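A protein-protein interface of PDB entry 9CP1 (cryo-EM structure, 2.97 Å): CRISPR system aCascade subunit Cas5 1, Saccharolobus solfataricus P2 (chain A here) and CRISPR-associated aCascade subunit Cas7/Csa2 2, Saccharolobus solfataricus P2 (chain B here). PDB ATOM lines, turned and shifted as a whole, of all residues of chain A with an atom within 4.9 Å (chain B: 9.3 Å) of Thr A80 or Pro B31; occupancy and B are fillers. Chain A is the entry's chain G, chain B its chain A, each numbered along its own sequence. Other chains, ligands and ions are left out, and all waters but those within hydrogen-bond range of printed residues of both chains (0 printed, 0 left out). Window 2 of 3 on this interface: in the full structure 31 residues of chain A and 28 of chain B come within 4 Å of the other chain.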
ATOM      1  N   VAL A  78       6.700 -24.196   9.958  1.00  0.00           N
ATOM      2  CA  VAL A  78       6.556 -25.644  10.066  1.00  0.00           C
ATOM      3  C   VAL A  78       7.807 -26.318   9.521  1.00  0.00           C
ATOM      4  O   VAL A  78       8.345 -25.907   8.487  1.00  0.00           O
ATOM      5  CB  VAL A  78       5.309 -26.160   9.315  1.00  0.00           C
ATOM      6  CG1 VAL A  78       5.025 -27.602   9.689  1.00  0.00           C
ATOM      7  CG2 VAL A  78       4.099 -25.288   9.604  1.00  0.00           C
ATOM      8  N   TYR A  79       8.260 -27.363  10.206  1.00  0.00           N
ATOM      9  CA  TYR A  79       9.380 -28.169   9.741  1.00  0.00           C
ATOM     10  C   TYR A  79       8.854 -29.372   8.970  1.00  0.00           C
ATOM     11  O   TYR A  79       8.002 -30.112   9.472  1.00  0.00           O
ATOM     12  CB  TYR A  79      10.243 -28.626  10.915  1.00  0.00           C
ATOM     13  CG  TYR A  79      11.259 -29.681  10.547  1.00  0.00           C
ATOM     14  CD1 TYR A  79      12.441 -29.339   9.911  1.00  0.00           C
ATOM     15  CD2 TYR A  79      11.038 -31.017  10.840  1.00  0.00           C
ATOM     16  CE1 TYR A  79      13.372 -30.297   9.572  1.00  0.00           C
ATOM     17  CE2 TYR A  79      11.963 -31.983  10.505  1.00  0.00           C
ATOM     18  CZ  TYR A  79      13.129 -31.616   9.872  1.00  0.00           C
ATOM     19  OH  TYR A  79      14.054 -32.576   9.536  1.00  0.00           O
ATOM     20  N   THR A  80       9.365 -29.567   7.756  1.00  0.00           N
ATOM     21  CA  THR A  80       8.854 -30.593   6.858  1.00  0.00           C
ATOM     22  C   THR A  80      10.006 -31.301   6.160  1.00  0.00           C
ATOM     23  O   THR A  80      10.958 -30.657   5.713  1.00  0.00           O
ATOM     24  CB  THR A  80       7.907 -29.988   5.814  1.00  0.00           C
ATOM     25  OG1 THR A  80       6.716 -29.535   6.463  1.00  0.00           O
ATOM     26  CG2 THR A  80       7.538 -31.010   4.752  1.00  0.00           C
ATOM     27  N   GLU A  81       9.910 -32.625   6.068  1.00  0.00           N
ATOM     28  CA  GLU A  81      10.866 -33.447   5.336  1.00  0.00           C
ATOM     29  C   GLU A  81      10.199 -33.923   4.051  1.00  0.00           C
ATOM     30  O   GLU A  81       9.231 -34.689   4.096  1.00  0.00           O
ATOM     31  CB  GLU A  81      11.329 -34.630   6.182  1.00  0.00           C
ATOM     32  CG  GLU A  81      12.233 -34.247   7.338  1.00  0.00           C
ATOM     33  CD  GLU A  81      12.782 -35.455   8.066  1.00  0.00           C
ATOM     34  OE1 GLU A  81      13.341 -36.350   7.397  1.00  0.00           O
ATOM     35  OE2 GLU A  81      12.656 -35.512   9.308  1.00  0.00           O
ATOM     36  N   ASP A  82      10.717 -33.472   2.913  1.00  0.00           N
ATOM     37  CA  ASP A  82      10.173 -33.859   1.615  1.00  0.00           C
ATOM     38  C   ASP A  82      11.162 -33.548   0.497  1.00  0.00           C
ATOM     39  O   ASP A  82      11.936 -34.410   0.079  1.00  0.00           O
ATOM     40  CB  ASP A  82       8.842 -33.148   1.353  1.00  0.00           C
ATOM     41  CG  ASP A  82       8.170 -33.621   0.078  1.00  0.00           C
ATOM     42  OD1 ASP A  82       7.395 -34.598   0.142  1.00  0.00           O
ATOM     43  OD2 ASP A  82       8.415 -33.018  -0.988  1.00  0.00           O
ATOM     44  N   THR A 109      15.636 -34.428   3.190  1.00  0.00           N
ATOM     45  CA  THR A 109      15.975 -33.020   3.032  1.00  0.00           C
ATOM     46  C   THR A 109      15.056 -32.164   3.896  1.00  0.00           C
ATOM     47  O   THR A 109      14.039 -31.654   3.425  1.00  0.00           O
ATOM     48  CB  THR A 109      15.869 -32.578   1.561  1.00  0.00           C
ATOM     49  OG1 THR A 109      16.666 -33.444   0.746  1.00  0.00           O
ATOM     50  CG2 THR A 109      16.372 -31.151   1.394  1.00  0.00           C
ATOM     51  N   GLY A 110      15.412 -32.024   5.169  1.00  0.00           N
ATOM     52  CA  GLY A 110      14.583 -31.258   6.081  1.00  0.00           C
ATOM     53  C   GLY A 110      14.606 -29.777   5.748  1.00  0.00           C
ATOM     54  O   GLY A 110      15.648 -29.202   5.432  1.00  0.00           O
ATOM     55  N   LYS A 111      13.432 -29.154   5.823  1.00  0.00           N
ATOM     56  CA  LYS A 111      13.287 -27.730   5.564  1.00  0.00           C
ATOM     57  C   LYS A 111      12.408 -27.117   6.640  1.00  0.00           C
ATOM     58  O   LYS A 111      11.622 -27.804   7.296  1.00  0.00           O
ATOM     59  CB  LYS A 111      12.684 -27.458   4.180  1.00  0.00           C
ATOM     60  CG  LYS A 111      13.518 -27.967   3.025  1.00  0.00           C
ATOM     61  CD  LYS A 111      12.796 -27.766   1.707  1.00  0.00           C
ATOM     62  CE  LYS A 111      13.636 -28.256   0.544  1.00  0.00           C
ATOM     63  NZ  LYS A 111      12.842 -28.336  -0.709  1.00  0.00           N
ATOM     64  N   TYR A 113       9.781 -24.171   6.673  1.00  0.00           N
ATOM     65  CA  TYR A 113       9.013 -23.188   5.923  1.00  0.00           C
ATOM     66  C   TYR A 113       8.469 -22.137   6.880  1.00  0.00           C
ATOM     67  O   TYR A 113       7.734 -22.462   7.821  1.00  0.00           O
ATOM     68  CB  TYR A 113       7.875 -23.861   5.163  1.00  0.00           C
ATOM     69  CG  TYR A 113       8.335 -24.769   4.048  1.00  0.00           C
ATOM     70  CD1 TYR A 113       8.596 -24.266   2.782  1.00  0.00           C
ATOM     71  CD2 TYR A 113       8.502 -26.128   4.259  1.00  0.00           C
ATOM     72  CE1 TYR A 113       9.015 -25.092   1.760  1.00  0.00           C
ATOM     73  CE2 TYR A 113       8.919 -26.962   3.244  1.00  0.00           C
ATOM     74  CZ  TYR A 113       9.174 -26.439   1.996  1.00  0.00           C
ATOM     75  OH  TYR A 113       9.591 -27.269   0.984  1.00  0.00           O
ATOM     76  N   ARG B  28       3.901 -30.840  -6.145  1.00  0.00           N
ATOM     77  CA  ARG B  28       4.765 -30.530  -5.014  1.00  0.00           C
ATOM     78  C   ARG B  28       4.096 -29.474  -4.143  1.00  0.00           C
ATOM     79  O   ARG B  28       3.717 -28.408  -4.637  1.00  0.00           O
ATOM     80  CB  ARG B  28       6.130 -30.047  -5.498  1.00  0.00           C
ATOM     81  CG  ARG B  28       7.181 -29.985  -4.413  1.00  0.00           C
ATOM     82  CD  ARG B  28       8.570 -29.862  -5.000  1.00  0.00           C
ATOM     83  NE  ARG B  28       9.328 -31.095  -4.836  1.00  0.00           N
ATOM     84  CZ  ARG B  28      10.453 -31.374  -5.477  1.00  0.00           C
ATOM     85  NH1 ARG B  28      10.983 -30.526  -6.342  1.00  0.00           N
ATOM     86  NH2 ARG B  28      11.062 -32.532  -5.246  1.00  0.00           N
ATOM     87  N   THR B  29       3.945 -29.771  -2.854  1.00  0.00           N
ATOM     88  CA  THR B  29       3.277 -28.876  -1.921  1.00  0.00           C
ATOM     89  C   THR B  29       4.110 -28.719  -0.656  1.00  0.00           C
ATOM     90  O   THR B  29       4.938 -29.567  -0.317  1.00  0.00           O
ATOM     91  CB  THR B  29       1.876 -29.379  -1.543  1.00  0.00           C
ATOM     92  OG1 THR B  29       1.990 -30.513  -0.675  1.00  0.00           O
ATOM     93  CG2 THR B  29       1.085 -29.769  -2.779  1.00  0.00           C
ATOM     94  N   ALA B  30       3.874 -27.610   0.038  1.00  0.00           N
ATOM     95  CA  ALA B  30       4.519 -27.287   1.299  1.00  0.00           C
ATOM     96  C   ALA B  30       3.491 -26.776   2.295  1.00  0.00           C
ATOM     97  O   ALA B  30       2.473 -26.200   1.901  1.00  0.00           O
ATOM     98  CB  ALA B  30       5.615 -26.230   1.103  1.00  0.00           C
ATOM     99  N   PRO B  31       3.726 -26.974   3.593  1.00  0.00           N
ATOM    100  CA  PRO B  31       2.773 -26.500   4.601  1.00  0.00           C
ATOM    101  C   PRO B  31       3.023 -25.060   5.016  1.00  0.00           C
ATOM    102  O   PRO B  31       4.162 -24.605   5.143  1.00  0.00           O
ATOM    103  CB  PRO B  31       3.019 -27.447   5.785  1.00  0.00           C
ATOM    104  CG  PRO B  31       3.964 -28.505   5.282  1.00  0.00           C
ATOM    105  CD  PRO B  31       4.729 -27.868   4.182  1.00  0.00           C
ATOM    106  N   VAL B  32       1.928 -24.332   5.236  1.00  0.00           N
ATOM    107  CA  VAL B  32       1.971 -22.971   5.750  1.00  0.00           C
ATOM    108  C   VAL B  32       0.962 -22.852   6.881  1.00  0.00           C
ATOM    109  O   VAL B  32      -0.001 -23.619   6.976  1.00  0.00           O
ATOM    110  CB  VAL B  32       1.680 -21.909   4.667  1.00  0.00           C
ATOM    111  CG1 VAL B  32       2.613 -22.075   3.484  1.00  0.00           C
ATOM    112  CG2 VAL B  32       0.231 -21.983   4.228  1.00  0.00           C
ATOM    113  N   VAL B  33       1.195 -21.871   7.747  1.00  0.00           N
ATOM    114  CA  VAL B  33       0.326 -21.586   8.883  1.00  0.00           C
ATOM    115  C   VAL B  33      -0.320 -20.228   8.657  1.00  0.00           C
ATOM    116  O   VAL B  33       0.376 -19.228   8.447  1.00  0.00           O
ATOM    117  CB  VAL B  33       1.100 -21.617  10.211  1.00  0.00           C
ATOM    118  CG1 VAL B  33       0.319 -20.897  11.293  1.00  0.00           C
ATOM    119  CG2 VAL B  33       1.387 -23.050  10.621  1.00  0.00           C
ATOM    120  N   LEU B  34      -1.647 -20.197   8.703  1.00  0.00           N
ATOM    121  CA  LEU B  34      -2.425 -18.991   8.475  1.00  0.00           C
ATOM    122  C   LEU B  34      -3.104 -18.583   9.774  1.00  0.00           C
ATOM    123  O   LEU B  34      -3.644 -19.429  10.497  1.00  0.00           O
ATOM    124  CB  LEU B  34      -3.464 -19.215   7.369  1.00  0.00           C
ATOM    125  CG  LEU B  34      -4.196 -18.009   6.775  1.00  0.00           C
ATOM    126  CD1 LEU B  34      -4.602 -18.308   5.345  1.00  0.00           C
ATOM    127  CD2 LEU B  34      -5.422 -17.632   7.591  1.00  0.00           C
ATOM    128  N   LEU B  41      -4.468 -22.123  11.274  1.00  0.00           N
ATOM    129  CA  LEU B  41      -4.836 -23.199  10.364  1.00  0.00           C
ATOM    130  C   LEU B  41      -3.613 -23.617   9.564  1.00  0.00           C
ATOM    131  O   LEU B  41      -2.841 -22.765   9.117  1.00  0.00           O
ATOM    132  CB  LEU B  41      -5.962 -22.772   9.419  1.00  0.00           C
ATOM    133  CG  LEU B  41      -7.294 -22.399  10.068  1.00  0.00           C
ATOM    134  CD1 LEU B  41      -8.242 -21.815   9.036  1.00  0.00           C
ATOM    135  CD2 LEU B  41      -7.913 -23.613  10.737  1.00  0.00           C
ATOM    136  N   VAL B  42      -3.435 -24.921   9.382  1.00  0.00           N
ATOM    137  CA  VAL B  42      -2.333 -25.458   8.592  1.00  0.00           C
ATOM    138  C   VAL B  42      -2.873 -25.829   7.219  1.00  0.00           C
ATOM    139  O   VAL B  42      -3.802 -26.638   7.107  1.00  0.00           O
ATOM    140  CB  VAL B  42      -1.686 -26.669   9.282  1.00  0.00           C
ATOM    141  CG1 VAL B  42      -0.403 -27.057   8.571  1.00  0.00           C
ATOM    142  CG2 VAL B  42      -1.417 -26.358  10.742  1.00  0.00           C
ATOM    143  N   ARG B  43      -2.295 -25.243   6.174  1.00  0.00           N
ATOM    144  CA  ARG B  43      -2.751 -25.463   4.810  1.00  0.00           C
ATOM    145  C   ARG B  43      -1.592 -25.911   3.935  1.00  0.00           C
ATOM    146  O   ARG B  43      -0.477 -25.397   4.053  1.00  0.00           O
ATOM    147  CB  ARG B  43      -3.376 -24.197   4.218  1.00  0.00           C
ATOM    148  CG  ARG B  43      -4.779 -23.903   4.704  1.00  0.00           C
ATOM    149  CD  ARG B  43      -5.806 -24.301   3.658  1.00  0.00           C
ATOM    150  NE  ARG B  43      -7.151 -24.377   4.214  1.00  0.00           N
ATOM    151  CZ  ARG B  43      -7.918 -23.326   4.469  1.00  0.00           C
ATOM    152  NH1 ARG B  43      -7.506 -22.094   4.223  1.00  0.00           N
ATOM    153  NH2 ARG B  43      -9.131 -23.517   4.981  1.00  0.00           N
ATOM    154  N   TYR B  44      -1.865 -26.857   3.044  1.00  0.00           N
ATOM    155  CA  TYR B  44      -0.870 -27.334   2.096  1.00  0.00           C
ATOM    156  C   TYR B  44      -1.027 -26.574   0.787  1.00  0.00           C
ATOM    157  O   TYR B  44      -2.127 -26.509   0.230  1.00  0.00           O
ATOM    158  CB  TYR B  44      -1.020 -28.836   1.872  1.00  0.00           C
ATOM    159  CG  TYR B  44      -0.408 -29.660   2.976  1.00  0.00           C
ATOM    160  CD1 TYR B  44      -1.022 -29.756   4.214  1.00  0.00           C
ATOM    161  CD2 TYR B  44       0.788 -30.333   2.784  1.00  0.00           C
ATOM    162  CE1 TYR B  44      -0.466 -30.503   5.230  1.00  0.00           C
ATOM    163  CE2 TYR B  44       1.353 -31.084   3.795  1.00  0.00           C
ATOM    164  CZ  TYR B  44       0.721 -31.166   5.016  1.00  0.00           C
ATOM    165  OH  TYR B  44       1.280 -31.912   6.026  1.00  0.00           O
ATOM    166  N   VAL B  45       0.067 -25.998   0.303  1.00  0.00           N
ATOM    167  CA  VAL B  45       0.014 -25.082  -0.832  1.00  0.00           C
ATOM    168  C   VAL B  45       1.023 -25.532  -1.882  1.00  0.00           C
ATOM    169  O   VAL B  45       2.152 -25.898  -1.529  1.00  0.00           O
ATOM    170  CB  VAL B  45       0.289 -23.639  -0.379  1.00  0.00           C
ATOM    171  CG1 VAL B  45      -0.037 -22.676  -1.477  1.00  0.00           C
ATOM    172  CG2 VAL B  45      -0.513 -23.302   0.860  1.00  0.00           C
ATOM    173  N   PRO B  46       0.669 -25.532  -3.166  1.00  0.00           N
ATOM    174  CA  PRO B  46       1.623 -25.957  -4.198  1.00  0.00           C
ATOM    175  C   PRO B  46       2.817 -25.021  -4.310  1.00  0.00           C
ATOM    176  O   PRO B  46       2.719 -23.816  -4.072  1.00  0.00           O
ATOM    177  CB  PRO B  46       0.787 -25.938  -5.483  1.00  0.00           C
ATOM    178  CG  PRO B  46      -0.366 -25.046  -5.180  1.00  0.00           C
ATOM    179  CD  PRO B  46      -0.660 -25.250  -3.733  1.00  0.00           C
ATOM    180  N   VAL B  47       3.961 -25.599  -4.684  1.00  0.00           N
ATOM    181  CA  VAL B  47       5.211 -24.868  -4.864  1.00  0.00           C
ATOM    182  C   VAL B  47       5.922 -25.399  -6.103  1.00  0.00           C
ATOM    183  O   VAL B  47       5.567 -26.440  -6.654  1.00  0.00           O
ATOM    184  CB  VAL B  47       6.142 -24.985  -3.638  1.00  0.00           C
ATOM    185  CG1 VAL B  47       5.542 -24.278  -2.440  1.00  0.00           C
ATOM    186  CG2 VAL B  47       6.408 -26.441  -3.325  1.00  0.00           C
ATOM    187  N   ILE B 143       6.677 -19.603  -4.512  1.00  0.00           N
ATOM    188  CA  ILE B 143       5.596 -19.839  -3.559  1.00  0.00           C
ATOM    189  C   ILE B 143       4.525 -18.775  -3.749  1.00  0.00           C
ATOM    190  O   ILE B 143       4.854 -17.590  -3.895  1.00  0.00           O
ATOM    191  CB  ILE B 143       6.126 -19.849  -2.116  1.00  0.00           C
ATOM    192  CG1 ILE B 143       7.077 -21.024  -1.912  1.00  0.00           C
ATOM    193  CG2 ILE B 143       4.991 -19.903  -1.114  1.00  0.00           C
ATOM    194  CD1 ILE B 143       7.569 -21.162  -0.499  1.00  0.00           C
ATOM    195  N   LEU B 146       1.311 -15.065   0.316  1.00  0.00           N
ATOM    196  CA  LEU B 146       0.477 -15.164   1.510  1.00  0.00           C
ATOM    197  C   LEU B 146       0.064 -13.750   1.905  1.00  0.00           C
ATOM    198  O   LEU B 146       0.593 -13.152   2.840  1.00  0.00           O
ATOM    199  CB  LEU B 146       1.221 -15.874   2.633  1.00  0.00           C
ATOM    200  CG  LEU B 146       1.800 -17.251   2.319  1.00  0.00           C
ATOM    201  CD1 LEU B 146       2.179 -17.957   3.604  1.00  0.00           C
ATOM    202  CD2 LEU B 146       0.807 -18.081   1.528  1.00  0.00           C
ATOM    203  N   ILE B 151      -5.520 -17.691   0.827  1.00  0.00           N
ATOM    204  CA  ILE B 151      -4.442 -18.194  -0.017  1.00  0.00           C
ATOM    205  C   ILE B 151      -5.016 -18.421  -1.413  1.00  0.00           C
ATOM    206  O   ILE B 151      -5.868 -19.308  -1.581  1.00  0.00           O
ATOM    207  CB  ILE B 151      -3.837 -19.483   0.549  1.00  0.00           C
ATOM    208  CG1 ILE B 151      -3.525 -19.308   2.033  1.00  0.00           C
ATOM    209  CG2 ILE B 151      -2.582 -19.852  -0.210  1.00  0.00           C
ATOM    210  CD1 ILE B 151      -2.904 -20.524   2.670  1.00  0.00           C
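Thr A80 touches just one residue of chain B: Pro B31 (3.2 Å).
Printed residues of chain A within 4 Å of Pro B31: Thr A80 and Tyr A113.
Gly A110 touches none of the printed residues of chain B.
Printed residues of chain B within 4 Å of Tyr A113: Ala B30 and Pro B31.
Printed residues of chain A within 4 Å of Ala B30: Tyr A113 (3.6 Å).
Printed residues of chain A within 4 Å of Val B33: Val A78 (3.7 Å).
The backbone NH of Ala B30 lies within hydrogen-bond range of the backbone carbonyl oxygen of Val B45, at 2.9 Å.
The backbone carbonyl oxygen (O) of Val A78 sits at hydrogen-bond distance from the backbone NH (N) of Tyr A113, at 2.9 Å.
O of Thr A80 lies within hydrogen-bond range of N of Lys A111, 2.9 Å away.
Val B33 touches Val A78.
OG1 of Thr A80 touches CG of Pro B31 (3.2 Å).
CE1 of Tyr A113 touches CB of Ala B30, at 3.6 Å.
O of Pro B31 touches CB of Tyr A113, 3.8 Å away.
Of the 9 printed residues of chain A, 3 touch a printed residue of chain B.
Hydrophobic or aromatic side chains of chain A within 4 Å of the printed part of chain B: Val A78 and Tyr A113.
Among the printed residues, no Asp or Glu carboxylate lies within 4 Å of a Lys or Arg side-chain nitrogen of the other chain.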
